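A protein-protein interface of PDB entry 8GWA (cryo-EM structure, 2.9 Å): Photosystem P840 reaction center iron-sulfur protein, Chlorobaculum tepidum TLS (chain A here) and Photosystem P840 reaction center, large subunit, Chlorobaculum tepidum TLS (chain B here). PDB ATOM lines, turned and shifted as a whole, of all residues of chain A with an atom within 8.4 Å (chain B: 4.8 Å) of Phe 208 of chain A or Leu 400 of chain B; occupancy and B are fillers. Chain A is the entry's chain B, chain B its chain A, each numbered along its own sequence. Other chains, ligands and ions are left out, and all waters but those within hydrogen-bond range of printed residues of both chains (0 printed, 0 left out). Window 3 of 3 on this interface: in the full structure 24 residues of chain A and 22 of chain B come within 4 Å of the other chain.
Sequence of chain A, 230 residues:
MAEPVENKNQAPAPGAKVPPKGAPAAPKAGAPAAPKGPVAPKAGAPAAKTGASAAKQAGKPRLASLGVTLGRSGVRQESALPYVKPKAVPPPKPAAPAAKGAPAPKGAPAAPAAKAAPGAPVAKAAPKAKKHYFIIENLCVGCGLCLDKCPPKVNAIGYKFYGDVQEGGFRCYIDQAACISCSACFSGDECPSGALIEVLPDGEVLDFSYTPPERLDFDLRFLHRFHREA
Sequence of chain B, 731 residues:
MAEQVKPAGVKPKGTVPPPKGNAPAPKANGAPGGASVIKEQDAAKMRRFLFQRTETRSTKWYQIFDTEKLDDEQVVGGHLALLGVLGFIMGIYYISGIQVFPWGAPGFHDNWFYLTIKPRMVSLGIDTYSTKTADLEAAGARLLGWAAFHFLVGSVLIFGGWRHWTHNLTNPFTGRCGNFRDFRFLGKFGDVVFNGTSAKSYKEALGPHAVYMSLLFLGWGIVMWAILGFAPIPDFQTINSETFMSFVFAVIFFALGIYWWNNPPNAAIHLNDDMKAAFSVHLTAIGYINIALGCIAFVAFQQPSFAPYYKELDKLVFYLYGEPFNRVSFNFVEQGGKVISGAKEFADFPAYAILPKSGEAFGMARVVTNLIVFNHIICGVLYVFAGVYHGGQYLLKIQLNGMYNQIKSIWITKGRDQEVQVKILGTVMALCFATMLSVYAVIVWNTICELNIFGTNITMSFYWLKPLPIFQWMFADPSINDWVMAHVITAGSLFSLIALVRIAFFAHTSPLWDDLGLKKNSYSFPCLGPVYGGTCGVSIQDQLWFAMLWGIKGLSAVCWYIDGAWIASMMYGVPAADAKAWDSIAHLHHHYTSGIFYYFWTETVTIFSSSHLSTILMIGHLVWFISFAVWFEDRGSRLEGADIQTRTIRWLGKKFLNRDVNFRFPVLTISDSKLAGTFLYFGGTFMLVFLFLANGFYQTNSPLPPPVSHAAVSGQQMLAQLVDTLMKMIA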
ATOM      1  N   CYS A 185      29.585  27.467 -25.240  1.00  0.00           N
ATOM      2  CA  CYS A 185      28.717  28.282 -24.395  1.00  0.00           C
ATOM      3  C   CYS A 185      28.729  27.795 -22.951  1.00  0.00           C
ATOM      4  O   CYS A 185      28.727  28.604 -22.016  1.00  0.00           O
ATOM      5  CB  CYS A 185      27.294  28.279 -24.953  1.00  0.00           C
ATOM      6  SG  CYS A 185      26.681  26.646 -25.421  1.00  0.00           S
ATOM      7  N   PHE A 186      28.744  26.478 -22.748  1.00  0.00           N
ATOM      8  CA  PHE A 186      28.663  25.917 -21.406  1.00  0.00           C
ATOM      9  C   PHE A 186      30.035  25.782 -20.753  1.00  0.00           C
ATOM     10  O   PHE A 186      30.217  26.186 -19.602  1.00  0.00           O
ATOM     11  CB  PHE A 186      27.967  24.556 -21.445  1.00  0.00           C
ATOM     12  CG  PHE A 186      27.592  24.030 -20.090  1.00  0.00           C
ATOM     13  CD1 PHE A 186      26.419  24.432 -19.477  1.00  0.00           C
ATOM     14  CD2 PHE A 186      28.424  23.155 -19.418  1.00  0.00           C
ATOM     15  CE1 PHE A 186      26.074  23.953 -18.232  1.00  0.00           C
ATOM     16  CE2 PHE A 186      28.083  22.672 -18.173  1.00  0.00           C
ATOM     17  CZ  PHE A 186      26.907  23.072 -17.581  1.00  0.00           C
ATOM     18  N   SER A 187      31.006  25.210 -21.469  1.00  0.00           N
ATOM     19  CA  SER A 187      32.336  25.015 -20.902  1.00  0.00           C
ATOM     20  C   SER A 187      33.056  26.325 -20.622  1.00  0.00           C
ATOM     21  O   SER A 187      34.040  26.320 -19.876  1.00  0.00           O
ATOM     22  CB  SER A 187      33.192  24.149 -21.829  1.00  0.00           C
ATOM     23  OG  SER A 187      33.191  24.659 -23.150  1.00  0.00           O
ATOM     24  N   GLY A 188      32.599  27.439 -21.195  1.00  0.00           N
ATOM     25  CA  GLY A 188      33.174  28.727 -20.857  1.00  0.00           C
ATOM     26  C   GLY A 188      32.925  29.144 -19.425  1.00  0.00           C
ATOM     27  O   GLY A 188      33.660  29.986 -18.899  1.00  0.00           O
ATOM     28  N   ASP A 189      31.906  28.568 -18.784  1.00  0.00           N
ATOM     29  CA  ASP A 189      31.595  28.819 -17.378  1.00  0.00           C
ATOM     30  C   ASP A 189      31.361  30.306 -17.118  1.00  0.00           C
ATOM     31  O   ASP A 189      32.008  30.934 -16.277  1.00  0.00           O
ATOM     32  CB  ASP A 189      32.690  28.257 -16.469  1.00  0.00           C
ATOM     33  CG  ASP A 189      32.576  26.763 -16.290  1.00  0.00           C
ATOM     34  OD1 ASP A 189      31.431  26.267 -16.290  1.00  0.00           O
ATOM     35  OD2 ASP A 189      33.618  26.090 -16.149  1.00  0.00           O
ATOM     36  N   GLU A 190      30.410  30.864 -17.864  1.00  0.00           N
ATOM     37  CA  GLU A 190      30.053  32.264 -17.720  1.00  0.00           C
ATOM     38  C   GLU A 190      28.574  32.524 -17.499  1.00  0.00           C
ATOM     39  O   GLU A 190      28.218  33.672 -17.215  1.00  0.00           O
ATOM     40  CB  GLU A 190      30.500  33.067 -18.948  1.00  0.00           C
ATOM     41  CG  GLU A 190      31.966  33.413 -18.957  1.00  0.00           C
ATOM     42  CD  GLU A 190      32.455  33.745 -20.342  1.00  0.00           C
ATOM     43  OE1 GLU A 190      32.872  32.819 -21.066  1.00  0.00           O
ATOM     44  OE2 GLU A 190      32.381  34.931 -20.716  1.00  0.00           O
ATOM     45  N   CYS A 191      27.709  31.529 -17.624  1.00  0.00           N
ATOM     46  CA  CYS A 191      26.292  31.773 -17.402  1.00  0.00           C
ATOM     47  C   CYS A 191      26.075  32.084 -15.929  1.00  0.00           C
ATOM     48  O   CYS A 191      26.275  31.202 -15.082  1.00  0.00           O
ATOM     49  CB  CYS A 191      25.459  30.570 -17.829  1.00  0.00           C
ATOM     50  SG  CYS A 191      23.674  30.818 -17.684  1.00  0.00           S
ATOM     51  N   PRO A 192      25.667  33.305 -15.576  1.00  0.00           N
ATOM     52  CA  PRO A 192      25.585  33.668 -14.155  1.00  0.00           C
ATOM     53  C   PRO A 192      24.342  33.152 -13.467  1.00  0.00           C
ATOM     54  O   PRO A 192      24.339  33.038 -12.235  1.00  0.00           O
ATOM     55  CB  PRO A 192      25.583  35.198 -14.195  1.00  0.00           C
ATOM     56  CG  PRO A 192      24.899  35.503 -15.488  1.00  0.00           C
ATOM     57  CD  PRO A 192      25.312  34.431 -16.455  1.00  0.00           C
ATOM     58  N   SER A 193      23.292  32.837 -14.219  1.00  0.00           N
ATOM     59  CA  SER A 193      22.020  32.418 -13.654  1.00  0.00           C
ATOM     60  C   SER A 193      21.757  30.932 -13.833  1.00  0.00           C
ATOM     61  O   SER A 193      20.685  30.452 -13.455  1.00  0.00           O
ATOM     62  CB  SER A 193      20.883  33.231 -14.269  1.00  0.00           C
ATOM     63  OG  SER A 193      21.011  33.295 -15.679  1.00  0.00           O
ATOM     64  N   GLY A 194      22.711  30.192 -14.387  1.00  0.00           N
ATOM     65  CA  GLY A 194      22.511  28.770 -14.592  1.00  0.00           C
ATOM     66  C   GLY A 194      21.400  28.438 -15.562  1.00  0.00           C
ATOM     67  O   GLY A 194      20.631  27.499 -15.325  1.00  0.00           O
ATOM     68  N   ALA A 195      21.293  29.194 -16.654  1.00  0.00           N
ATOM     69  CA  ALA A 195      20.304  28.899 -17.680  1.00  0.00           C
ATOM     70  C   ALA A 195      20.819  27.879 -18.686  1.00  0.00           C
ATOM     71  O   ALA A 195      20.052  27.032 -19.156  1.00  0.00           O
ATOM     72  CB  ALA A 195      19.889  30.182 -18.399  1.00  0.00           C
ATOM     73  N   LEU A 196      22.102  27.947 -19.032  1.00  0.00           N
ATOM     74  CA  LEU A 196      22.722  26.884 -19.807  1.00  0.00           C
ATOM     75  C   LEU A 196      22.785  25.619 -18.962  1.00  0.00           C
ATOM     76  O   LEU A 196      23.138  25.670 -17.780  1.00  0.00           O
ATOM     77  CB  LEU A 196      24.124  27.295 -20.248  1.00  0.00           C
ATOM     78  CG  LEU A 196      24.208  28.186 -21.484  1.00  0.00           C
ATOM     79  CD1 LEU A 196      25.503  28.970 -21.467  1.00  0.00           C
ATOM     80  CD2 LEU A 196      24.097  27.356 -22.749  1.00  0.00           C
ATOM     81  N   ILE A 197      22.442  24.479 -19.564  1.00  0.00           N
ATOM     82  CA  ILE A 197      22.274  23.238 -18.826  1.00  0.00           C
ATOM     83  C   ILE A 197      23.135  22.106 -19.377  1.00  0.00           C
ATOM     84  O   ILE A 197      23.765  21.380 -18.604  1.00  0.00           O
ATOM     85  CB  ILE A 197      20.789  22.821 -18.762  1.00  0.00           C
ATOM     86  CG1 ILE A 197      20.139  22.883 -20.141  1.00  0.00           C
ATOM     87  CG2 ILE A 197      20.043  23.695 -17.772  1.00  0.00           C
ATOM     88  CD1 ILE A 197      18.767  22.262 -20.195  1.00  0.00           C
ATOM     89  N   GLU A 198      23.185  21.932 -20.700  1.00  0.00           N
ATOM     90  CA  GLU A 198      23.892  20.804 -21.315  1.00  0.00           C
ATOM     91  C   GLU A 198      23.328  19.469 -20.816  1.00  0.00           C
ATOM     92  O   GLU A 198      23.944  18.750 -20.026  1.00  0.00           O
ATOM     93  CB  GLU A 198      25.408  20.856 -21.075  1.00  0.00           C
ATOM     94  CG  GLU A 198      26.151  19.717 -21.787  1.00  0.00           C
ATOM     95  CD  GLU A 198      27.654  19.763 -21.612  1.00  0.00           C
ATOM     96  OE1 GLU A 198      28.151  20.666 -20.916  1.00  0.00           O
ATOM     97  OE2 GLU A 198      28.344  18.885 -22.170  1.00  0.00           O
ATOM     98  N   VAL A 205      21.009  16.239 -16.741  1.00  0.00           N
ATOM     99  CA  VAL A 205      20.996  17.679 -16.957  1.00  0.00           C
ATOM    100  C   VAL A 205      22.021  18.309 -16.029  1.00  0.00           C
ATOM    101  O   VAL A 205      21.865  18.271 -14.803  1.00  0.00           O
ATOM    102  CB  VAL A 205      19.606  18.282 -16.720  1.00  0.00           C
ATOM    103  CG1 VAL A 205      19.626  19.762 -17.048  1.00  0.00           C
ATOM    104  CG2 VAL A 205      18.562  17.551 -17.547  1.00  0.00           C
ATOM    105  N   LEU A 206      23.059  18.896 -16.610  1.00  0.00           N
ATOM    106  CA  LEU A 206      24.009  19.681 -15.842  1.00  0.00           C
ATOM    107  C   LEU A 206      23.470  21.093 -15.651  1.00  0.00           C
ATOM    108  O   LEU A 206      22.427  21.468 -16.186  1.00  0.00           O
ATOM    109  CB  LEU A 206      25.368  19.723 -16.540  1.00  0.00           C
ATOM    110  CG  LEU A 206      26.263  18.488 -16.467  1.00  0.00           C
ATOM    111  CD1 LEU A 206      27.438  18.646 -17.416  1.00  0.00           C
ATOM    112  CD2 LEU A 206      26.747  18.262 -15.051  1.00  0.00           C
ATOM    113  N   ASP A 207      24.185  21.874 -14.853  1.00  0.00           N
ATOM    114  CA  ASP A 207      23.884  23.288 -14.706  1.00  0.00           C
ATOM    115  C   ASP A 207      25.125  24.159 -14.804  1.00  0.00           C
ATOM    116  O   ASP A 207      25.034  25.285 -15.307  1.00  0.00           O
ATOM    117  CB  ASP A 207      23.190  23.536 -13.356  1.00  0.00           C
ATOM    118  CG  ASP A 207      22.642  24.938 -13.213  1.00  0.00           C
ATOM    119  OD1 ASP A 207      22.805  25.762 -14.130  1.00  0.00           O
ATOM    120  OD2 ASP A 207      22.036  25.216 -12.163  1.00  0.00           O
ATOM    121  N   PHE A 208      26.285  23.655 -14.401  1.00  0.00           N
ATOM    122  CA  PHE A 208      27.539  24.383 -14.471  1.00  0.00           C
ATOM    123  C   PHE A 208      28.628  23.321 -14.508  1.00  0.00           C
ATOM    124  O   PHE A 208      28.432  22.204 -14.022  1.00  0.00           O
ATOM    125  CB  PHE A 208      27.682  25.340 -13.279  1.00  0.00           C
ATOM    126  CG  PHE A 208      28.856  26.272 -13.370  1.00  0.00           C
ATOM    127  CD1 PHE A 208      28.807  27.379 -14.199  1.00  0.00           C
ATOM    128  CD2 PHE A 208      29.991  26.062 -12.611  1.00  0.00           C
ATOM    129  CE1 PHE A 208      29.873  28.249 -14.279  1.00  0.00           C
ATOM    130  CE2 PHE A 208      31.062  26.928 -12.688  1.00  0.00           C
ATOM    131  CZ  PHE A 208      31.002  28.023 -13.520  1.00  0.00           C
ATOM    132  N   SER A 209      29.773  23.663 -15.107  1.00  0.00           N
ATOM    133  CA  SER A 209      30.754  22.632 -15.439  1.00  0.00           C
ATOM    134  C   SER A 209      31.213  21.872 -14.202  1.00  0.00           C
ATOM    135  O   SER A 209      31.345  20.643 -14.235  1.00  0.00           O
ATOM    136  CB  SER A 209      31.947  23.247 -16.166  1.00  0.00           C
ATOM    137  OG  SER A 209      31.655  23.452 -17.537  1.00  0.00           O
ATOM    138  N   TYR A 210      31.460  22.577 -13.101  1.00  0.00           N
ATOM    139  CA  TYR A 210      31.710  21.924 -11.826  1.00  0.00           C
ATOM    140  C   TYR A 210      30.922  22.637 -10.739  1.00  0.00           C
ATOM    141  O   TYR A 210      30.791  23.863 -10.750  1.00  0.00           O
ATOM    142  CB  TYR A 210      33.201  21.903 -11.460  1.00  0.00           C
ATOM    143  CG  TYR A 210      33.435  21.481 -10.029  1.00  0.00           C
ATOM    144  CD1 TYR A 210      33.357  20.145  -9.664  1.00  0.00           C
ATOM    145  CD2 TYR A 210      33.704  22.416  -9.039  1.00  0.00           C
ATOM    146  CE1 TYR A 210      33.552  19.748  -8.358  1.00  0.00           C
ATOM    147  CE2 TYR A 210      33.900  22.028  -7.728  1.00  0.00           C
ATOM    148  CZ  TYR A 210      33.824  20.692  -7.395  1.00  0.00           C
ATOM    149  OH  TYR A 210      34.018  20.295  -6.093  1.00  0.00           O
ATOM    150  N   THR A 211      30.410  21.859  -9.789  1.00  0.00           N
ATOM    151  CA  THR A 211      29.615  22.379  -8.694  1.00  0.00           C
ATOM    152  C   THR A 211      30.311  22.107  -7.367  1.00  0.00           C
ATOM    153  O   THR A 211      30.824  20.998  -7.160  1.00  0.00           O
ATOM    154  CB  THR A 211      28.214  21.746  -8.690  1.00  0.00           C
ATOM    155  OG1 THR A 211      27.637  21.859  -9.996  1.00  0.00           O
ATOM    156  CG2 THR A 211      27.313  22.439  -7.683  1.00  0.00           C
ATOM    157  N   PRO A 212      30.372  23.082  -6.462  1.00  0.00           N
ATOM    158  CA  PRO A 212      30.991  22.860  -5.148  1.00  0.00           C
ATOM    159  C   PRO A 212      30.357  21.686  -4.422  1.00  0.00           C
ATOM    160  O   PRO A 212      29.230  21.277  -4.741  1.00  0.00           O
ATOM    161  CB  PRO A 212      30.727  24.185  -4.419  1.00  0.00           C
ATOM    162  CG  PRO A 212      30.729  25.193  -5.508  1.00  0.00           C
ATOM    163  CD  PRO A 212      30.136  24.514  -6.722  1.00  0.00           C
ATOM    164  N   PRO A 213      31.049  21.118  -3.427  1.00  0.00           N
ATOM    165  CA  PRO A 213      30.666  19.792  -2.920  1.00  0.00           C
ATOM    166  C   PRO A 213      29.550  19.757  -1.882  1.00  0.00           C
ATOM    167  O   PRO A 213      29.410  18.740  -1.198  1.00  0.00           O
ATOM    168  CB  PRO A 213      31.976  19.269  -2.317  1.00  0.00           C
ATOM    169  CG  PRO A 213      32.719  20.490  -1.925  1.00  0.00           C
ATOM    170  CD  PRO A 213      32.371  21.541  -2.931  1.00  0.00           C
ATOM    171  N   LEU B 396      37.805  34.576  -5.649  1.00  0.00           N
ATOM    172  CA  LEU B 396      36.797  34.124  -6.600  1.00  0.00           C
ATOM    173  C   LEU B 396      37.228  32.833  -7.279  1.00  0.00           C
ATOM    174  O   LEU B 396      36.403  31.942  -7.512  1.00  0.00           O
ATOM    175  CB  LEU B 396      36.523  35.207  -7.644  1.00  0.00           C
ATOM    176  CG  LEU B 396      35.783  34.701  -8.886  1.00  0.00           C
ATOM    177  CD1 LEU B 396      34.370  34.287  -8.545  1.00  0.00           C
ATOM    178  CD2 LEU B 396      35.769  35.739  -9.974  1.00  0.00           C
ATOM    179  N   LYS B 397      38.516  32.715  -7.614  1.00  0.00           N
ATOM    180  CA  LYS B 397      38.992  31.477  -8.220  1.00  0.00           C
ATOM    181  C   LYS B 397      38.770  30.284  -7.299  1.00  0.00           C
ATOM    182  O   LYS B 397      38.448  29.189  -7.773  1.00  0.00           O
ATOM    183  CB  LYS B 397      40.470  31.592  -8.587  1.00  0.00           C
ATOM    184  CG  LYS B 397      40.923  30.537  -9.587  1.00  0.00           C
ATOM    185  CD  LYS B 397      42.412  30.625  -9.860  1.00  0.00           C
ATOM    186  CE  LYS B 397      43.212  29.947  -8.762  1.00  0.00           C
ATOM    187  NZ  LYS B 397      42.976  28.478  -8.723  1.00  0.00           N
ATOM    188  N   ILE B 398      38.938  30.470  -5.990  1.00  0.00           N
ATOM    189  CA  ILE B 398      38.691  29.369  -5.062  1.00  0.00           C
ATOM    190  C   ILE B 398      37.218  29.238  -4.673  1.00  0.00           C
ATOM    191  O   ILE B 398      36.814  28.179  -4.173  1.00  0.00           O
ATOM    192  CB  ILE B 398      39.559  29.478  -3.796  1.00  0.00           C
ATOM    193  CG1 ILE B 398      39.133  30.656  -2.924  1.00  0.00           C
ATOM    194  CG2 ILE B 398      41.024  29.586  -4.168  1.00  0.00           C
ATOM    195  CD1 ILE B 398      39.617  30.543  -1.499  1.00  0.00           C
ATOM    196  N   GLN B 399      36.408  30.280  -4.876  1.00  0.00           N
ATOM    197  CA  GLN B 399      34.965  30.136  -4.703  1.00  0.00           C
ATOM    198  C   GLN B 399      34.343  29.379  -5.867  1.00  0.00           C
ATOM    199  O   GLN B 399      33.330  28.693  -5.691  1.00  0.00           O
ATOM    200  CB  GLN B 399      34.299  31.508  -4.556  1.00  0.00           C
ATOM    201  CG  GLN B 399      34.622  32.222  -3.256  1.00  0.00           C
ATOM    202  CD  GLN B 399      33.895  33.539  -3.086  1.00  0.00           C
ATOM    203  OE1 GLN B 399      32.668  33.581  -3.029  1.00  0.00           O
ATOM    204  NE2 GLN B 399      34.653  34.626  -2.997  1.00  0.00           N
ATOM    205  N   LEU B 400      34.936  29.489  -7.056  1.00  0.00           N
ATOM    206  CA  LEU B 400      34.364  28.851  -8.236  1.00  0.00           C
ATOM    207  C   LEU B 400      34.605  27.348  -8.246  1.00  0.00           C
ATOM    208  O   LEU B 400      33.768  26.594  -8.753  1.00  0.00           O
ATOM    209  CB  LEU B 400      34.939  29.487  -9.499  1.00  0.00           C
ATOM    210  CG  LEU B 400      34.124  30.642 -10.074  1.00  0.00           C
ATOM    211  CD1 LEU B 400      34.945  31.432 -11.077  1.00  0.00           C
ATOM    212  CD2 LEU B 400      32.861  30.102 -10.714  1.00  0.00           C
ATOM    213  N   ASN B 401      35.732  26.895  -7.702  1.00  0.00           N
ATOM    214  CA  ASN B 401      36.062  25.479  -7.673  1.00  0.00           C
ATOM    215  C   ASN B 401      35.751  24.830  -6.331  1.00  0.00           C
ATOM    216  O   ASN B 401      36.121  23.675  -6.115  1.00  0.00           O
ATOM    217  CB  ASN B 401      37.536  25.268  -8.037  1.00  0.00           C
ATOM    218  CG  ASN B 401      38.485  25.966  -7.079  1.00  0.00           C
ATOM    219  OD1 ASN B 401      38.081  26.458  -6.030  1.00  0.00           O
ATOM    220  ND2 ASN B 401      39.761  26.011  -7.443  1.00  0.00           N
ATOM    221  N   GLY B 402      35.087  25.544  -5.427  1.00  0.00           N
ATOM    222  CA  GLY B 402      34.724  24.991  -4.141  1.00  0.00           C
ATOM    223  C   GLY B 402      35.817  24.997  -3.097  1.00  0.00           C
ATOM    224  O   GLY B 402      35.578  24.531  -1.975  1.00  0.00           O
ATOM    225  N   HIS B 508      32.376  36.374  -5.633  1.00  0.00           N
ATOM    226  CA  HIS B 508      31.587  35.424  -6.407  1.00  0.00           C
ATOM    227  C   HIS B 508      30.090  35.625  -6.254  1.00  0.00           C
ATOM    228  O   HIS B 508      29.351  35.490  -7.229  1.00  0.00           O
ATOM    229  CB  HIS B 508      31.947  33.991  -6.003  1.00  0.00           C
ATOM    230  CG  HIS B 508      31.222  32.938  -6.779  1.00  0.00           C
ATOM    231  ND1 HIS B 508      31.378  32.776  -8.139  1.00  0.00           N
ATOM    232  CD2 HIS B 508      30.344  31.985  -6.385  1.00  0.00           C
ATOM    233  CE1 HIS B 508      30.625  31.772  -8.549  1.00  0.00           C
ATOM    234  NE2 HIS B 508      29.986  31.275  -7.506  1.00  0.00           N
ATOM    235  N   LYS B 519      25.285  34.662 -10.010  1.00  0.00           N
ATOM    236  CA  LYS B 519      26.582  34.539  -9.358  1.00  0.00           C
ATOM    237  C   LYS B 519      27.656  35.130 -10.263  1.00  0.00           C
ATOM    238  O   LYS B 519      27.557  35.071 -11.491  1.00  0.00           O
ATOM    239  CB  LYS B 519      26.911  33.081  -9.011  1.00  0.00           C
ATOM    240  CG  LYS B 519      27.200  32.183 -10.202  1.00  0.00           C
ATOM    241  CD  LYS B 519      27.410  30.746  -9.752  1.00  0.00           C
ATOM    242  CE  LYS B 519      27.829  29.854 -10.905  1.00  0.00           C
ATOM    243  NZ  LYS B 519      26.678  29.481 -11.768  1.00  0.00           N
ATOM    244  N   ASN B 521      31.350  35.130 -11.796  1.00  0.00           N
ATOM    245  CA  ASN B 521      32.325  34.084 -12.081  1.00  0.00           C
ATOM    246  C   ASN B 521      33.394  34.520 -13.082  1.00  0.00           C
ATOM    247  O   ASN B 521      33.931  33.683 -13.815  1.00  0.00           O
ATOM    248  CB  ASN B 521      31.626  32.826 -12.596  1.00  0.00           C
ATOM    249  CG  ASN B 521      30.598  33.127 -13.668  1.00  0.00           C
ATOM    250  OD1 ASN B 521      30.480  34.262 -14.128  1.00  0.00           O
ATOM    251  ND2 ASN B 521      29.844  32.111 -14.066  1.00  0.00           N
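O of Asp 189 of chain A sits at hydrogen-bond distance from ND2 of Asn 521 of chain B (3.3 Å).
The backbone NH of Lys 519 of chain B sits at hydrogen-bond distance from the backbone carbonyl oxygen of Pro 192 of chain A.
The side-chain sulfur of Cys 191 of chain A sits close to the backbone NH of Leu 196 of chain A (3.5 Å).
The backbone NH of Gly 194 of chain A lies close to the side-chain sulfur of Cys 191 of chain A (3.5 Å).
The side-chain sulfur of Cys 191 of chain A lies close to the backbone NH of Ala 195 of chain A.
The backbone carbonyl oxygen (O) of Lys 397 of chain B sits close to the side-chain amide oxygen (OD1) of Asn 401 of chain B.
The side-chain amide oxygen (OD1) of Asn 401 of chain B sits close to the backbone carbonyl oxygen (O) of Ile 398 of chain B.
The side-chain hydroxyl (OG) of Ser 209 of chain A lies close to the side-chain carboxylate (OD1) of Asp 189 of chain A (3.1 Å).
Asn 521 of chain B touches Glu 190 of chain A.
Cys 191 of chain A touches Lys 519 of chain B (O to NZ, 3.8 Å).
Cys 191 of chain A touches Asn 521 of chain B (O to ND2, 3.8 Å).
Leu 400 of chain B touches Phe 208 of chain A (CD2 to CZ, 3.96 Å).
Lys 519 of chain B touches Phe 208 of chain A (NZ to CD1, 3.9 Å).
Phe 208 of chain A touches Asn 521 of chain B (CE1 to ND2, 3.9 Å).
Asn 401 of chain B touches Tyr 210 of chain A.
Of the printed residues of chain B, Glu 190 of chain A touches Asn 521.
Of the printed residues of chain B, Cys 191 of chain A touches Lys 519 and Asn 521.
Of the printed residues of chain B, Pro 192 of chain A touches Lys 519.
Phe 208 of chain A touches just these residues of chain B: Leu 400, Lys 519 and Asn 521.
Leu 400 of chain B touches just one residue of chain A: Phe 208 (3.96 Å).
The nearest printed residue of chain B that does not touch Phe 208 of chain A is His 508 of chain B (6.2 Å).
The nearest residue of chain A that does not touch Leu 400 of chain B is Tyr 210 of chain A (4.2 Å).
The nearest printed residue of chain A that does not touch Lys 519 of chain B is Gly 194 of chain A (4.8 Å).
Hydrophobic or aromatic side chains of chain A within 4 Å of the printed part of chain B: Pro 192, Phe 208 and Tyr 210.
Printed residues of chain B that touch a printed residue of chain A: Leu 400, Asn 401, Lys 519 and Asn 521.
Hydrophobic or aromatic side chains of chain B within 4 Å of the printed part of chain A: Leu 400.
Among the printed residues, no Asp or Glu carboxylate lies within 4 Å of a Lys or Arg side-chain nitrogen of the other chain.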
